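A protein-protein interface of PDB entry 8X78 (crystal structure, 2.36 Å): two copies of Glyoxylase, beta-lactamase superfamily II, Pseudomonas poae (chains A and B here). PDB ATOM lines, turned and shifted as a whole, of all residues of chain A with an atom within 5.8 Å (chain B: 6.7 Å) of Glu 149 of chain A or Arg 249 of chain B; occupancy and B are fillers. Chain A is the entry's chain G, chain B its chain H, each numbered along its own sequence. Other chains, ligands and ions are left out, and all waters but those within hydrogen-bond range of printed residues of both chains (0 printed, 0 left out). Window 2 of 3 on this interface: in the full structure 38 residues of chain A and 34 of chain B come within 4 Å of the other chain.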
ATOM      1  N   GLN A 143      -8.511   5.014 -19.645  1.00  0.00           N
ATOM      2  CA  GLN A 143      -9.479   4.810 -18.577  1.00  0.00           C
ATOM      3  C   GLN A 143      -9.286   5.782 -17.425  1.00  0.00           C
ATOM      4  O   GLN A 143     -10.156   5.873 -16.558  1.00  0.00           O
ATOM      5  CB  GLN A 143      -9.347   3.402 -18.032  1.00  0.00           C
ATOM      6  CG  GLN A 143      -8.204   3.285 -16.990  1.00  0.00           C
ATOM      7  CD  GLN A 143      -7.984   1.872 -16.526  1.00  0.00           C
ATOM      8  OE1 GLN A 143      -8.889   1.095 -16.455  1.00  0.00           O
ATOM      9  NE2 GLN A 143      -6.765   1.513 -16.322  1.00  0.00           N
ATOM     10  N   HIS A 144      -8.137   6.446 -17.360  1.00  0.00           N
ATOM     11  CA  HIS A 144      -7.895   7.474 -16.357  1.00  0.00           C
ATOM     12  C   HIS A 144      -8.541   8.793 -16.770  1.00  0.00           C
ATOM     13  O   HIS A 144      -8.561   9.156 -17.950  1.00  0.00           O
ATOM     14  CB  HIS A 144      -6.393   7.662 -16.146  1.00  0.00           C
ATOM     15  CG  HIS A 144      -5.717   6.447 -15.601  1.00  0.00           C
ATOM     16  ND1 HIS A 144      -5.899   6.017 -14.303  1.00  0.00           N
ATOM     17  CD2 HIS A 144      -4.912   5.532 -16.190  1.00  0.00           C
ATOM     18  CE1 HIS A 144      -5.205   4.910 -14.104  1.00  0.00           C
ATOM     19  NE2 HIS A 144      -4.598   4.593 -15.235  1.00  0.00           N
ATOM     20  N   GLU A 145      -9.091   9.506 -15.788  1.00  0.00           N
ATOM     21  CA  GLU A 145      -9.888  10.690 -16.094  1.00  0.00           C
ATOM     22  C   GLU A 145      -9.045  11.916 -16.410  1.00  0.00           C
ATOM     23  O   GLU A 145      -9.493  12.791 -17.160  1.00  0.00           O
ATOM     24  CB  GLU A 145     -10.799  11.003 -14.914  1.00  0.00           C
ATOM     25  CG  GLU A 145     -11.828   9.942 -14.747  1.00  0.00           C
ATOM     26  CD  GLU A 145     -12.724   9.889 -15.952  1.00  0.00           C
ATOM     27  OE1 GLU A 145     -13.042  10.972 -16.489  1.00  0.00           O
ATOM     28  OE2 GLU A 145     -13.062   8.770 -16.394  1.00  0.00           O
ATOM     29  N   THR A 146      -7.844  12.003 -15.856  1.00  0.00           N
ATOM     30  CA  THR A 146      -6.968  13.142 -16.051  1.00  0.00           C
ATOM     31  C   THR A 146      -5.689  12.725 -16.759  1.00  0.00           C
ATOM     32  O   THR A 146      -5.291  11.555 -16.738  1.00  0.00           O
ATOM     33  CB  THR A 146      -6.642  13.817 -14.714  1.00  0.00           C
ATOM     34  OG1 THR A 146      -5.326  13.420 -14.297  1.00  0.00           O
ATOM     35  CG2 THR A 146      -7.685  13.493 -13.657  1.00  0.00           C
ATOM     36  N   GLU A 147      -5.048  13.708 -17.394  1.00  0.00           N
ATOM     37  CA  GLU A 147      -3.778  13.459 -18.068  1.00  0.00           C
ATOM     38  C   GLU A 147      -2.632  13.260 -17.085  1.00  0.00           C
ATOM     39  O   GLU A 147      -1.637  12.627 -17.449  1.00  0.00           O
ATOM     40  CB  GLU A 147      -3.466  14.602 -19.056  1.00  0.00           C
ATOM     41  CG  GLU A 147      -4.457  14.710 -20.199  1.00  0.00           C
ATOM     42  CD  GLU A 147      -4.494  13.480 -21.092  1.00  0.00           C
ATOM     43  OE1 GLU A 147      -3.419  12.940 -21.447  1.00  0.00           O
ATOM     44  OE2 GLU A 147      -5.617  13.041 -21.419  1.00  0.00           O
ATOM     45  N   GLU A 148      -2.771  13.774 -15.857  1.00  0.00           N
ATOM     46  CA  GLU A 148      -1.765  13.552 -14.823  1.00  0.00           C
ATOM     47  C   GLU A 148      -1.615  12.064 -14.551  1.00  0.00           C
ATOM     48  O   GLU A 148      -0.499  11.571 -14.329  1.00  0.00           O
ATOM     49  CB  GLU A 148      -2.150  14.262 -13.503  1.00  0.00           C
ATOM     50  CG  GLU A 148      -2.148  15.804 -13.536  1.00  0.00           C
ATOM     51  CD  GLU A 148      -2.606  16.431 -12.226  1.00  0.00           C
ATOM     52  OE1 GLU A 148      -3.104  15.702 -11.349  1.00  0.00           O
ATOM     53  OE2 GLU A 148      -2.555  17.686 -12.121  1.00  0.00           O
ATOM     54  N   GLU A 149      -2.725  11.334 -14.598  1.00  0.00           N
ATOM     55  CA  GLU A 149      -2.712   9.893 -14.412  1.00  0.00           C
ATOM     56  C   GLU A 149      -2.131   9.151 -15.608  1.00  0.00           C
ATOM     57  O   GLU A 149      -1.746   7.980 -15.480  1.00  0.00           O
ATOM     58  CB  GLU A 149      -4.141   9.402 -14.170  1.00  0.00           C
ATOM     59  CG  GLU A 149      -4.716   9.804 -12.818  1.00  0.00           C
ATOM     60  CD  GLU A 149      -6.237   9.666 -12.776  1.00  0.00           C
ATOM     61  OE1 GLU A 149      -6.758   8.524 -12.723  1.00  0.00           O
ATOM     62  OE2 GLU A 149      -6.908  10.724 -12.830  1.00  0.00           O
ATOM     63  N   LYS A 150      -2.039   9.812 -16.762  1.00  0.00           N
ATOM     64  CA  LYS A 150      -1.459   9.232 -17.961  1.00  0.00           C
ATOM     65  C   LYS A 150      -0.014   9.648 -18.156  1.00  0.00           C
ATOM     66  O   LYS A 150       0.661   9.095 -19.031  1.00  0.00           O
ATOM     67  CB  LYS A 150      -2.270   9.641 -19.195  1.00  0.00           C
ATOM     68  CG  LYS A 150      -3.737   9.301 -19.126  1.00  0.00           C
ATOM     69  CD  LYS A 150      -4.489   9.966 -20.244  1.00  0.00           C
ATOM     70  CE  LYS A 150      -5.986   9.731 -20.114  1.00  0.00           C
ATOM     71  NZ  LYS A 150      -6.808  10.435 -21.157  1.00  0.00           N
ATOM     72  N   GLU A 151       0.488  10.567 -17.332  1.00  0.00           N
ATOM     73  CA  GLU A 151       1.765  11.200 -17.625  1.00  0.00           C
ATOM     74  C   GLU A 151       2.886  10.175 -17.743  1.00  0.00           C
ATOM     75  O   GLU A 151       3.689  10.227 -18.678  1.00  0.00           O
ATOM     76  CB  GLU A 151       2.074  12.233 -16.551  1.00  0.00           C
ATOM     77  CG  GLU A 151       3.178  13.204 -16.911  1.00  0.00           C
ATOM     78  CD  GLU A 151       3.282  14.326 -15.893  1.00  0.00           C
ATOM     79  OE1 GLU A 151       2.232  14.665 -15.297  1.00  0.00           O
ATOM     80  OE2 GLU A 151       4.390  14.880 -15.695  1.00  0.00           O
ATOM     81  N   TRP A 152       2.963   9.228 -16.805  1.00  0.00           N
ATOM     82  CA  TRP A 152       4.076   8.280 -16.827  1.00  0.00           C
ATOM     83  C   TRP A 152       4.074   7.423 -18.086  1.00  0.00           C
ATOM     84  O   TRP A 152       5.132   7.182 -18.676  1.00  0.00           O
ATOM     85  CB  TRP A 152       4.058   7.393 -15.586  1.00  0.00           C
ATOM     86  CG  TRP A 152       5.201   6.439 -15.573  1.00  0.00           C
ATOM     87  CD1 TRP A 152       6.455   6.652 -15.078  1.00  0.00           C
ATOM     88  CD2 TRP A 152       5.207   5.124 -16.137  1.00  0.00           C
ATOM     89  NE1 TRP A 152       7.233   5.535 -15.269  1.00  0.00           N
ATOM     90  CE2 TRP A 152       6.491   4.587 -15.927  1.00  0.00           C
ATOM     91  CE3 TRP A 152       4.244   4.344 -16.786  1.00  0.00           C
ATOM     92  CZ2 TRP A 152       6.834   3.297 -16.332  1.00  0.00           C
ATOM     93  CZ3 TRP A 152       4.583   3.086 -17.202  1.00  0.00           C
ATOM     94  CH2 TRP A 152       5.868   2.561 -16.964  1.00  0.00           C
ATOM     95  N   VAL A 153       2.900   6.948 -18.506  1.00  0.00           N
ATOM     96  CA  VAL A 153       2.794   6.134 -19.716  1.00  0.00           C
ATOM     97  C   VAL A 153       3.331   6.879 -20.937  1.00  0.00           C
ATOM     98  O   VAL A 153       3.896   6.261 -21.854  1.00  0.00           O
ATOM     99  CB  VAL A 153       1.332   5.700 -19.939  1.00  0.00           C
ATOM    100  CG1 VAL A 153       1.154   5.112 -21.347  1.00  0.00           C
ATOM    101  CG2 VAL A 153       0.887   4.713 -18.859  1.00  0.00           C
ATOM    102  N   ILE B 213      -6.655  -2.662   1.697  1.00  0.00           N
ATOM    103  CA  ILE B 213      -5.603  -3.241   0.881  1.00  0.00           C
ATOM    104  C   ILE B 213      -4.276  -2.997   1.569  1.00  0.00           C
ATOM    105  O   ILE B 213      -3.852  -1.845   1.714  1.00  0.00           O
ATOM    106  CB  ILE B 213      -5.589  -2.650  -0.540  1.00  0.00           C
ATOM    107  CG1 ILE B 213      -6.719  -3.266  -1.365  1.00  0.00           C
ATOM    108  CG2 ILE B 213      -4.229  -2.871  -1.175  1.00  0.00           C
ATOM    109  CD1 ILE B 213      -6.922  -2.638  -2.729  1.00  0.00           C
ATOM    110  N   ASN B 224       2.648   6.937  -5.698  1.00  0.00           N
ATOM    111  CA  ASN B 224       2.797   5.952  -6.763  1.00  0.00           C
ATOM    112  C   ASN B 224       1.452   5.650  -7.406  1.00  0.00           C
ATOM    113  O   ASN B 224       1.329   5.616  -8.637  1.00  0.00           O
ATOM    114  CB  ASN B 224       3.424   4.663  -6.225  1.00  0.00           C
ATOM    115  CG  ASN B 224       4.852   4.850  -5.773  1.00  0.00           C
ATOM    116  OD1 ASN B 224       5.326   4.158  -4.863  1.00  0.00           O
ATOM    117  ND2 ASN B 224       5.550   5.791  -6.400  1.00  0.00           N
ATOM    118  N   ILE B 225       0.425   5.434  -6.582  1.00  0.00           N
ATOM    119  CA  ILE B 225      -0.893   5.081  -7.102  1.00  0.00           C
ATOM    120  C   ILE B 225      -1.662   6.323  -7.532  1.00  0.00           C
ATOM    121  O   ILE B 225      -2.414   6.280  -8.514  1.00  0.00           O
ATOM    122  CB  ILE B 225      -1.691   4.263  -6.068  1.00  0.00           C
ATOM    123  CG1 ILE B 225      -2.645   3.303  -6.783  1.00  0.00           C
ATOM    124  CG2 ILE B 225      -2.490   5.187  -5.148  1.00  0.00           C
ATOM    125  CD1 ILE B 225      -3.104   2.140  -5.940  1.00  0.00           C
ATOM    126  N   GLU B 226      -1.486   7.445  -6.835  1.00  0.00           N
ATOM    127  CA  GLU B 226      -2.255   8.639  -7.175  1.00  0.00           C
ATOM    128  C   GLU B 226      -1.739   9.290  -8.452  1.00  0.00           C
ATOM    129  O   GLU B 226      -2.529   9.687  -9.314  1.00  0.00           O
ATOM    130  CB  GLU B 226      -2.228   9.624  -6.017  1.00  0.00           C
ATOM    131  CG  GLU B 226      -3.027   9.142  -4.848  1.00  0.00           C
ATOM    132  CD  GLU B 226      -2.726   9.928  -3.609  1.00  0.00           C
ATOM    133  OE1 GLU B 226      -2.104  11.006  -3.725  1.00  0.00           O
ATOM    134  OE2 GLU B 226      -3.105   9.465  -2.512  1.00  0.00           O
ATOM    135  N   ARG B 227      -0.420   9.419  -8.579  1.00  0.00           N
ATOM    136  CA  ARG B 227       0.249   9.924  -9.770  1.00  0.00           C
ATOM    137  C   ARG B 227       0.489   8.846 -10.831  1.00  0.00           C
ATOM    138  O   ARG B 227       1.124   9.135 -11.853  1.00  0.00           O
ATOM    139  CB  ARG B 227       1.587  10.561  -9.374  1.00  0.00           C
ATOM    140  CG  ARG B 227       1.502  11.937  -8.727  1.00  0.00           C
ATOM    141  CD  ARG B 227       2.253  12.953  -9.583  1.00  0.00           C
ATOM    142  NE  ARG B 227       1.874  12.794 -10.983  1.00  0.00           N
ATOM    143  CZ  ARG B 227       2.465  13.386 -12.013  1.00  0.00           C
ATOM    144  NH1 ARG B 227       3.480  14.219 -11.847  1.00  0.00           N
ATOM    145  NH2 ARG B 227       2.029  13.127 -13.244  1.00  0.00           N
ATOM    146  N   MET B 228       0.007   7.620 -10.616  1.00  0.00           N
ATOM    147  CA  MET B 228       0.211   6.509 -11.555  1.00  0.00           C
ATOM    148  C   MET B 228       1.666   6.434 -12.019  1.00  0.00           C
ATOM    149  O   MET B 228       1.962   6.345 -13.211  1.00  0.00           O
ATOM    150  CB  MET B 228      -0.736   6.620 -12.750  1.00  0.00           C
ATOM    151  CG  MET B 228      -2.176   6.319 -12.411  1.00  0.00           C
ATOM    152  SD  MET B 228      -2.354   4.752 -11.551  1.00  0.00           S
ATOM    153  CE  MET B 228      -2.240   3.585 -12.923  1.00  0.00           C
ATOM    154  N   TRP B 229       2.586   6.463 -11.059  1.00  0.00           N
ATOM    155  CA  TRP B 229       4.002   6.646 -11.365  1.00  0.00           C
ATOM    156  C   TRP B 229       4.860   5.664 -10.568  1.00  0.00           C
ATOM    157  O   TRP B 229       5.102   5.857  -9.364  1.00  0.00           O
ATOM    158  CB  TRP B 229       4.415   8.089 -11.095  1.00  0.00           C
ATOM    159  CG  TRP B 229       5.659   8.480 -11.787  1.00  0.00           C
ATOM    160  CD1 TRP B 229       6.886   7.924 -11.624  1.00  0.00           C
ATOM    161  CD2 TRP B 229       5.817   9.521 -12.763  1.00  0.00           C
ATOM    162  NE1 TRP B 229       7.804   8.540 -12.436  1.00  0.00           N
ATOM    163  CE2 TRP B 229       7.174   9.531 -13.143  1.00  0.00           C
ATOM    164  CE3 TRP B 229       4.944  10.442 -13.352  1.00  0.00           C
ATOM    165  CZ2 TRP B 229       7.681  10.422 -14.081  1.00  0.00           C
ATOM    166  CZ3 TRP B 229       5.450  11.331 -14.286  1.00  0.00           C
ATOM    167  CH2 TRP B 229       6.804  11.315 -14.643  1.00  0.00           C
ATOM    168  N   ILE B 242       1.660  -0.549 -12.906  1.00  0.00           N
ATOM    169  CA  ILE B 242       0.580   0.301 -13.387  1.00  0.00           C
ATOM    170  C   ILE B 242      -0.728  -0.486 -13.399  1.00  0.00           C
ATOM    171  O   ILE B 242      -1.770   0.001 -12.944  1.00  0.00           O
ATOM    172  CB  ILE B 242       0.948   0.879 -14.774  1.00  0.00           C
ATOM    173  CG1 ILE B 242       1.965   2.028 -14.623  1.00  0.00           C
ATOM    174  CG2 ILE B 242      -0.297   1.296 -15.587  1.00  0.00           C
ATOM    175  CD1 ILE B 242       1.355   3.351 -14.127  1.00  0.00           C
ATOM    176  N   VAL B 244      -1.452  -3.193 -11.577  1.00  0.00           N
ATOM    177  CA  VAL B 244      -1.940  -3.483 -10.233  1.00  0.00           C
ATOM    178  C   VAL B 244      -2.513  -2.221  -9.599  1.00  0.00           C
ATOM    179  O   VAL B 244      -3.471  -2.289  -8.818  1.00  0.00           O
ATOM    180  CB  VAL B 244      -0.835  -4.115  -9.363  1.00  0.00           C
ATOM    181  CG1 VAL B 244      -1.326  -4.287  -7.918  1.00  0.00           C
ATOM    182  CG2 VAL B 244      -0.430  -5.461  -9.937  1.00  0.00           C
ATOM    183  N   TYR B 245      -1.946  -1.056  -9.919  1.00  0.00           N
ATOM    184  CA  TYR B 245      -2.505   0.186  -9.398  1.00  0.00           C
ATOM    185  C   TYR B 245      -3.968   0.310  -9.785  1.00  0.00           C
ATOM    186  O   TYR B 245      -4.789   0.798  -8.998  1.00  0.00           O
ATOM    187  CB  TYR B 245      -1.720   1.392  -9.914  1.00  0.00           C
ATOM    188  CG  TYR B 245      -0.289   1.498  -9.428  1.00  0.00           C
ATOM    189  CD1 TYR B 245       0.180   0.724  -8.365  1.00  0.00           C
ATOM    190  CD2 TYR B 245       0.591   2.392 -10.024  1.00  0.00           C
ATOM    191  CE1 TYR B 245       1.488   0.840  -7.929  1.00  0.00           C
ATOM    192  CE2 TYR B 245       1.895   2.505  -9.601  1.00  0.00           C
ATOM    193  CZ  TYR B 245       2.339   1.734  -8.554  1.00  0.00           C
ATOM    194  OH  TYR B 245       3.643   1.869  -8.142  1.00  0.00           O
ATOM    195  N   ARG B 246      -4.309  -0.131 -10.999  1.00  0.00           N
ATOM    196  CA  ARG B 246      -5.690  -0.061 -11.468  1.00  0.00           C
ATOM    197  C   ARG B 246      -6.562  -1.115 -10.784  1.00  0.00           C
ATOM    198  O   ARG B 246      -7.716  -0.840 -10.429  1.00  0.00           O
ATOM    199  CB  ARG B 246      -5.720  -0.213 -12.993  1.00  0.00           C
ATOM    200  CG  ARG B 246      -5.020   0.922 -13.757  1.00  0.00           C
ATOM    201  CD  ARG B 246      -4.202   0.464 -15.006  1.00  0.00           C
ATOM    202  NE  ARG B 246      -3.774   1.619 -15.799  1.00  0.00           N
ATOM    203  CZ  ARG B 246      -3.394   1.580 -17.068  1.00  0.00           C
ATOM    204  NH1 ARG B 246      -3.363   0.448 -17.747  1.00  0.00           N
ATOM    205  NH2 ARG B 246      -3.036   2.709 -17.671  1.00  0.00           N
ATOM    206  N   GLN B 247      -6.023  -2.319 -10.565  1.00  0.00           N
ATOM    207  CA  GLN B 247      -6.778  -3.340  -9.842  1.00  0.00           C
ATOM    208  C   GLN B 247      -7.085  -2.901  -8.411  1.00  0.00           C
ATOM    209  O   GLN B 247      -8.170  -3.181  -7.886  1.00  0.00           O
ATOM    210  CB  GLN B 247      -6.009  -4.662  -9.829  1.00  0.00           C
ATOM    211  CG  GLN B 247      -5.928  -5.393 -11.160  1.00  0.00           C
ATOM    212  CD  GLN B 247      -5.247  -6.756 -11.020  1.00  0.00           C
ATOM    213  OE1 GLN B 247      -4.281  -6.914 -10.262  1.00  0.00           O
ATOM    214  NE2 GLN B 247      -5.758  -7.747 -11.742  1.00  0.00           N
ATOM    215  N   MET B 248      -6.132  -2.223  -7.761  1.00  0.00           N
ATOM    216  CA  MET B 248      -6.338  -1.696  -6.414  1.00  0.00           C
ATOM    217  C   MET B 248      -7.324  -0.533  -6.409  1.00  0.00           C
ATOM    218  O   MET B 248      -8.283  -0.527  -5.630  1.00  0.00           O
ATOM    219  CB  MET B 248      -4.999  -1.267  -5.815  1.00  0.00           C
ATOM    220  CG  MET B 248      -4.018  -2.414  -5.710  1.00  0.00           C
ATOM    221  SD  MET B 248      -2.475  -1.956  -4.916  1.00  0.00           S
ATOM    222  CE  MET B 248      -1.675  -3.539  -4.743  1.00  0.00           C
ATOM    223  N   ARG B 249      -7.091   0.469  -7.265  1.00  0.00           N
ATOM    224  CA  ARG B 249      -8.024   1.585  -7.389  1.00  0.00           C
ATOM    225  C   ARG B 249      -9.454   1.092  -7.508  1.00  0.00           C
ATOM    226  O   ARG B 249     -10.370   1.648  -6.893  1.00  0.00           O
ATOM    227  CB  ARG B 249      -7.672   2.436  -8.611  1.00  0.00           C
ATOM    228  CG  ARG B 249      -6.570   3.455  -8.402  1.00  0.00           C
ATOM    229  CD  ARG B 249      -6.217   4.095  -9.730  1.00  0.00           C
ATOM    230  NE  ARG B 249      -5.310   5.218  -9.564  1.00  0.00           N
ATOM    231  CZ  ARG B 249      -5.658   6.487  -9.704  1.00  0.00           C
ATOM    232  NH1 ARG B 249      -6.883   6.830 -10.060  1.00  0.00           N
ATOM    233  NH2 ARG B 249      -4.751   7.433  -9.483  1.00  0.00           N
ATOM    234  N   SER B 250      -9.663   0.046  -8.304  1.00  0.00           N
ATOM    235  CA  SER B 250     -11.005  -0.489  -8.499  1.00  0.00           C
ATOM    236  C   SER B 250     -11.542  -1.136  -7.223  1.00  0.00           C
ATOM    237  O   SER B 250     -12.729  -0.999  -6.904  1.00  0.00           O
ATOM    238  CB  SER B 250     -10.985  -1.483  -9.660  1.00  0.00           C
ATOM    239  OG  SER B 250     -12.273  -2.000  -9.927  1.00  0.00           O
ATOM    240  N   VAL B 251     -10.684  -1.826  -6.467  1.00  0.00           N
ATOM    241  CA  VAL B 251     -11.162  -2.541  -5.285  1.00  0.00           C
ATOM    242  C   VAL B 251     -11.609  -1.579  -4.187  1.00  0.00           C
ATOM    243  O   VAL B 251     -12.449  -1.933  -3.352  1.00  0.00           O
ATOM    244  CB  VAL B 251     -10.083  -3.511  -4.767  1.00  0.00           C
ATOM    245  CG1 VAL B 251     -10.234  -3.736  -3.278  1.00  0.00           C
ATOM    246  CG2 VAL B 251     -10.171  -4.836  -5.504  1.00  0.00           C
ATOM    247  N   VAL B 252     -11.068  -0.363  -4.157  1.00  0.00           N
ATOM    248  CA  VAL B 252     -11.366   0.586  -3.091  1.00  0.00           C
ATOM    249  C   VAL B 252     -12.071   1.828  -3.627  1.00  0.00           C
ATOM    250  O   VAL B 252     -12.133   2.841  -2.936  1.00  0.00           O
ATOM    251  CB  VAL B 252     -10.100   0.970  -2.309  1.00  0.00           C
ATOM    252  CG1 VAL B 252      -9.307  -0.281  -1.895  1.00  0.00           C
ATOM    253  CG2 VAL B 252      -9.247   1.935  -3.122  1.00  0.00           C
ATOM    254  N   LYS B 253     -12.585   1.768  -4.858  1.00  0.00           N
ATOM    255  CA  LYS B 253     -13.322   2.881  -5.465  1.00  0.00           C
ATOM    256  C   LYS B 253     -12.539   4.189  -5.369  1.00  0.00           C
ATOM    257  O   LYS B 253     -13.097   5.257  -5.103  1.00  0.00           O
ATOM    258  CB  LYS B 253     -14.705   3.036  -4.833  1.00  0.00           C
ATOM    259  CG  LYS B 253     -15.443   1.725  -4.629  1.00  0.00           C
ATOM    260  CD  LYS B 253     -16.310   1.345  -5.821  1.00  0.00           C
ATOM    261  CE  LYS B 253     -16.865  -0.069  -5.653  1.00  0.00           C
ATOM    262  NZ  LYS B 253     -17.349  -0.355  -4.258  1.00  0.00           N
ATOM    263  N   ASN B 254     -11.225   4.098  -5.579  1.00  0.00           N
ATOM    264  CA  ASN B 254     -10.321   5.248  -5.604  1.00  0.00           C
ATOM    265  C   ASN B 254     -10.285   6.003  -4.276  1.00  0.00           C
ATOM    266  O   ASN B 254      -9.864   7.165  -4.230  1.00  0.00           O
ATOM    267  CB  ASN B 254     -10.668   6.198  -6.755  1.00  0.00           C
ATOM    268  CG  ASN B 254     -10.455   5.555  -8.114  1.00  0.00           C
ATOM    269  OD1 ASN B 254      -9.345   5.563  -8.659  1.00  0.00           O
ATOM    270  ND2 ASN B 254     -11.514   4.975  -8.661  1.00  0.00           N
ATOM    271  N   LYS B 255     -10.700   5.364  -3.182  1.00  0.00           N
ATOM    272  CA  LYS B 255     -10.498   5.912  -1.841  1.00  0.00           C
ATOM    273  C   LYS B 255      -9.112   5.479  -1.379  1.00  0.00           C
ATOM    274  O   LYS B 255      -8.926   4.371  -0.871  1.00  0.00           O
ATOM    275  CB  LYS B 255     -11.594   5.448  -0.888  1.00  0.00           C
ATOM    276  CG  LYS B 255     -12.973   5.957  -1.276  1.00  0.00           C
ATOM    277  CD  LYS B 255     -13.839   6.198  -0.057  1.00  0.00           C
ATOM    278  CE  LYS B 255     -15.081   6.994  -0.427  1.00  0.00           C
ATOM    279  NZ  LYS B 255     -15.912   7.275   0.773  1.00  0.00           N
ATOM    280  N   PHE B 256      -8.132   6.367  -1.554  1.00  0.00           N
ATOM    281  CA  PHE B 256      -6.737   5.955  -1.450  1.00  0.00           C
ATOM    282  C   PHE B 256      -6.354   5.579  -0.022  1.00  0.00           C
ATOM    283  O   PHE B 256      -5.482   4.723   0.172  1.00  0.00           O
ATOM    284  CB  PHE B 256      -5.821   7.060  -1.986  1.00  0.00           C
ATOM    285  CG  PHE B 256      -6.129   7.485  -3.412  1.00  0.00           C
ATOM    286  CD1 PHE B 256      -7.108   8.435  -3.674  1.00  0.00           C
ATOM    287  CD2 PHE B 256      -5.428   6.947  -4.484  1.00  0.00           C
ATOM    288  CE1 PHE B 256      -7.392   8.834  -4.975  1.00  0.00           C
ATOM    289  CE2 PHE B 256      -5.706   7.340  -5.792  1.00  0.00           C
ATOM    290  CZ  PHE B 256      -6.690   8.284  -6.037  1.00  0.00           C
ATOM    291  N   ILE B 259      -5.942   2.036   1.028  1.00  0.00           N
ATOM    292  CA  ILE B 259      -4.713   1.356   0.649  1.00  0.00           C
ATOM    293  C   ILE B 259      -3.641   1.766   1.643  1.00  0.00           C
ATOM    294  O   ILE B 259      -3.510   2.953   1.968  1.00  0.00           O
ATOM    295  CB  ILE B 259      -4.303   1.707  -0.791  1.00  0.00           C
ATOM    296  CG1 ILE B 259      -5.390   1.248  -1.753  1.00  0.00           C
ATOM    297  CG2 ILE B 259      -2.970   1.070  -1.152  1.00  0.00           C
ATOM    298  CD1 ILE B 259      -5.062   1.514  -3.176  1.00  0.00           C
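Hydrophobic or aromatic side chains of chain A that line the printed part of chain B: His 144 and Trp 152. Printed residues of chain B that touch a printed residue of chain A: Arg 227, Met 228, Trp 229, Ile 242, Arg 246 and Arg 249. Hydrophobic or aromatic side chains of chain B that line the printed part of chain A: Met 228, Trp 229 and Ile 242. Among the printed residues, Asp or Glu carboxylates within 4 Å of a Lys or Arg side-chain nitrogen of the other chain: Glu 149 of chain A with Arg 249 of chain B (3.2 Å) and Glu 151 of chain A with Arg 227 of chain B (2.6 Å).
The backbone carbonyl oxygen (O) of Ile 225 of chain B lies within hydrogen-bond range of the guanidinium group (NH2) of Arg 249 of chain B (2.8 Å). OE1 of Glu 149 of chain A is in hydrogen-bond range of ND1 of His 144 of chain A (3.1 Å). N of Trp 229 of chain B sits at hydrogen-bond distance from O of Asn 224 of chain B (2.9 Å). NE of Arg 249 of chain B is in hydrogen-bond range of SD of Met 228 of chain B (3.6 Å). O of Glu 226 of chain B lies within hydrogen-bond range of NH2 of Arg 249 of chain B, 3.2 Å away. The backbone NH (N) of Glu 149 of chain A lies within hydrogen-bond range of the side-chain hydroxyl (OG1) of Thr 146 of chain A, 3.3 Å away.
Among the printed residues, merely in contact across the chains: Glu 149 of chain A with Met 228 of chain B (3.2 Å), Trp 152 of chain A with Met 228 of chain B (3.3 Å), His 144 of chain A with Met 228 of chain B (3.5 Å), Trp 152 of chain A with Trp 229 of chain B (3.5 Å), Trp 152 of chain A with Ile 242 of chain B (3.8 Å) and Glu 151 of chain A with Trp 229 of chain B (3.9 Å).
No position is printed for both chains. Of the 11 pairs that touch across the chains among the printed residues, none has its exchanged pair printed and touching as well.
Of chain B, only Met 228 and Arg 249 come within 4 Å of Glu 149 of chain A. Arg 249 of chain B touches just one residue of chain A: Glu 149. Of the printed residues of chain B, Trp 152 of chain A touches Met 228, Trp 229 and Ile 242. Of the printed residues of chain B, Gln 143 of chain A touches Arg 246 (3.0 Å). Val 252 of chain B touches none of the printed residues of chain A.
OE1 of Glu 151 of chain A is in salt-bridge range of NH2 of Arg 227 of chain B, at 2.6 Å. O of Glu 148 of chain A lies within hydrogen-bond range of NH2 of Arg 227 of chain B (3.2 Å). NE of Arg 246 of chain B lies close to NE2 of Gln 143 of chain A. NE2 of His 144 of chain A sits at hydrogen-bond distance from NE of Arg 246 of chain B (3.1 Å). The side-chain carboxylate (OE1) of Glu 149 of chain A lies within salt-bridge range of the guanidinium group (NH1) of Arg 249 of chain B.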
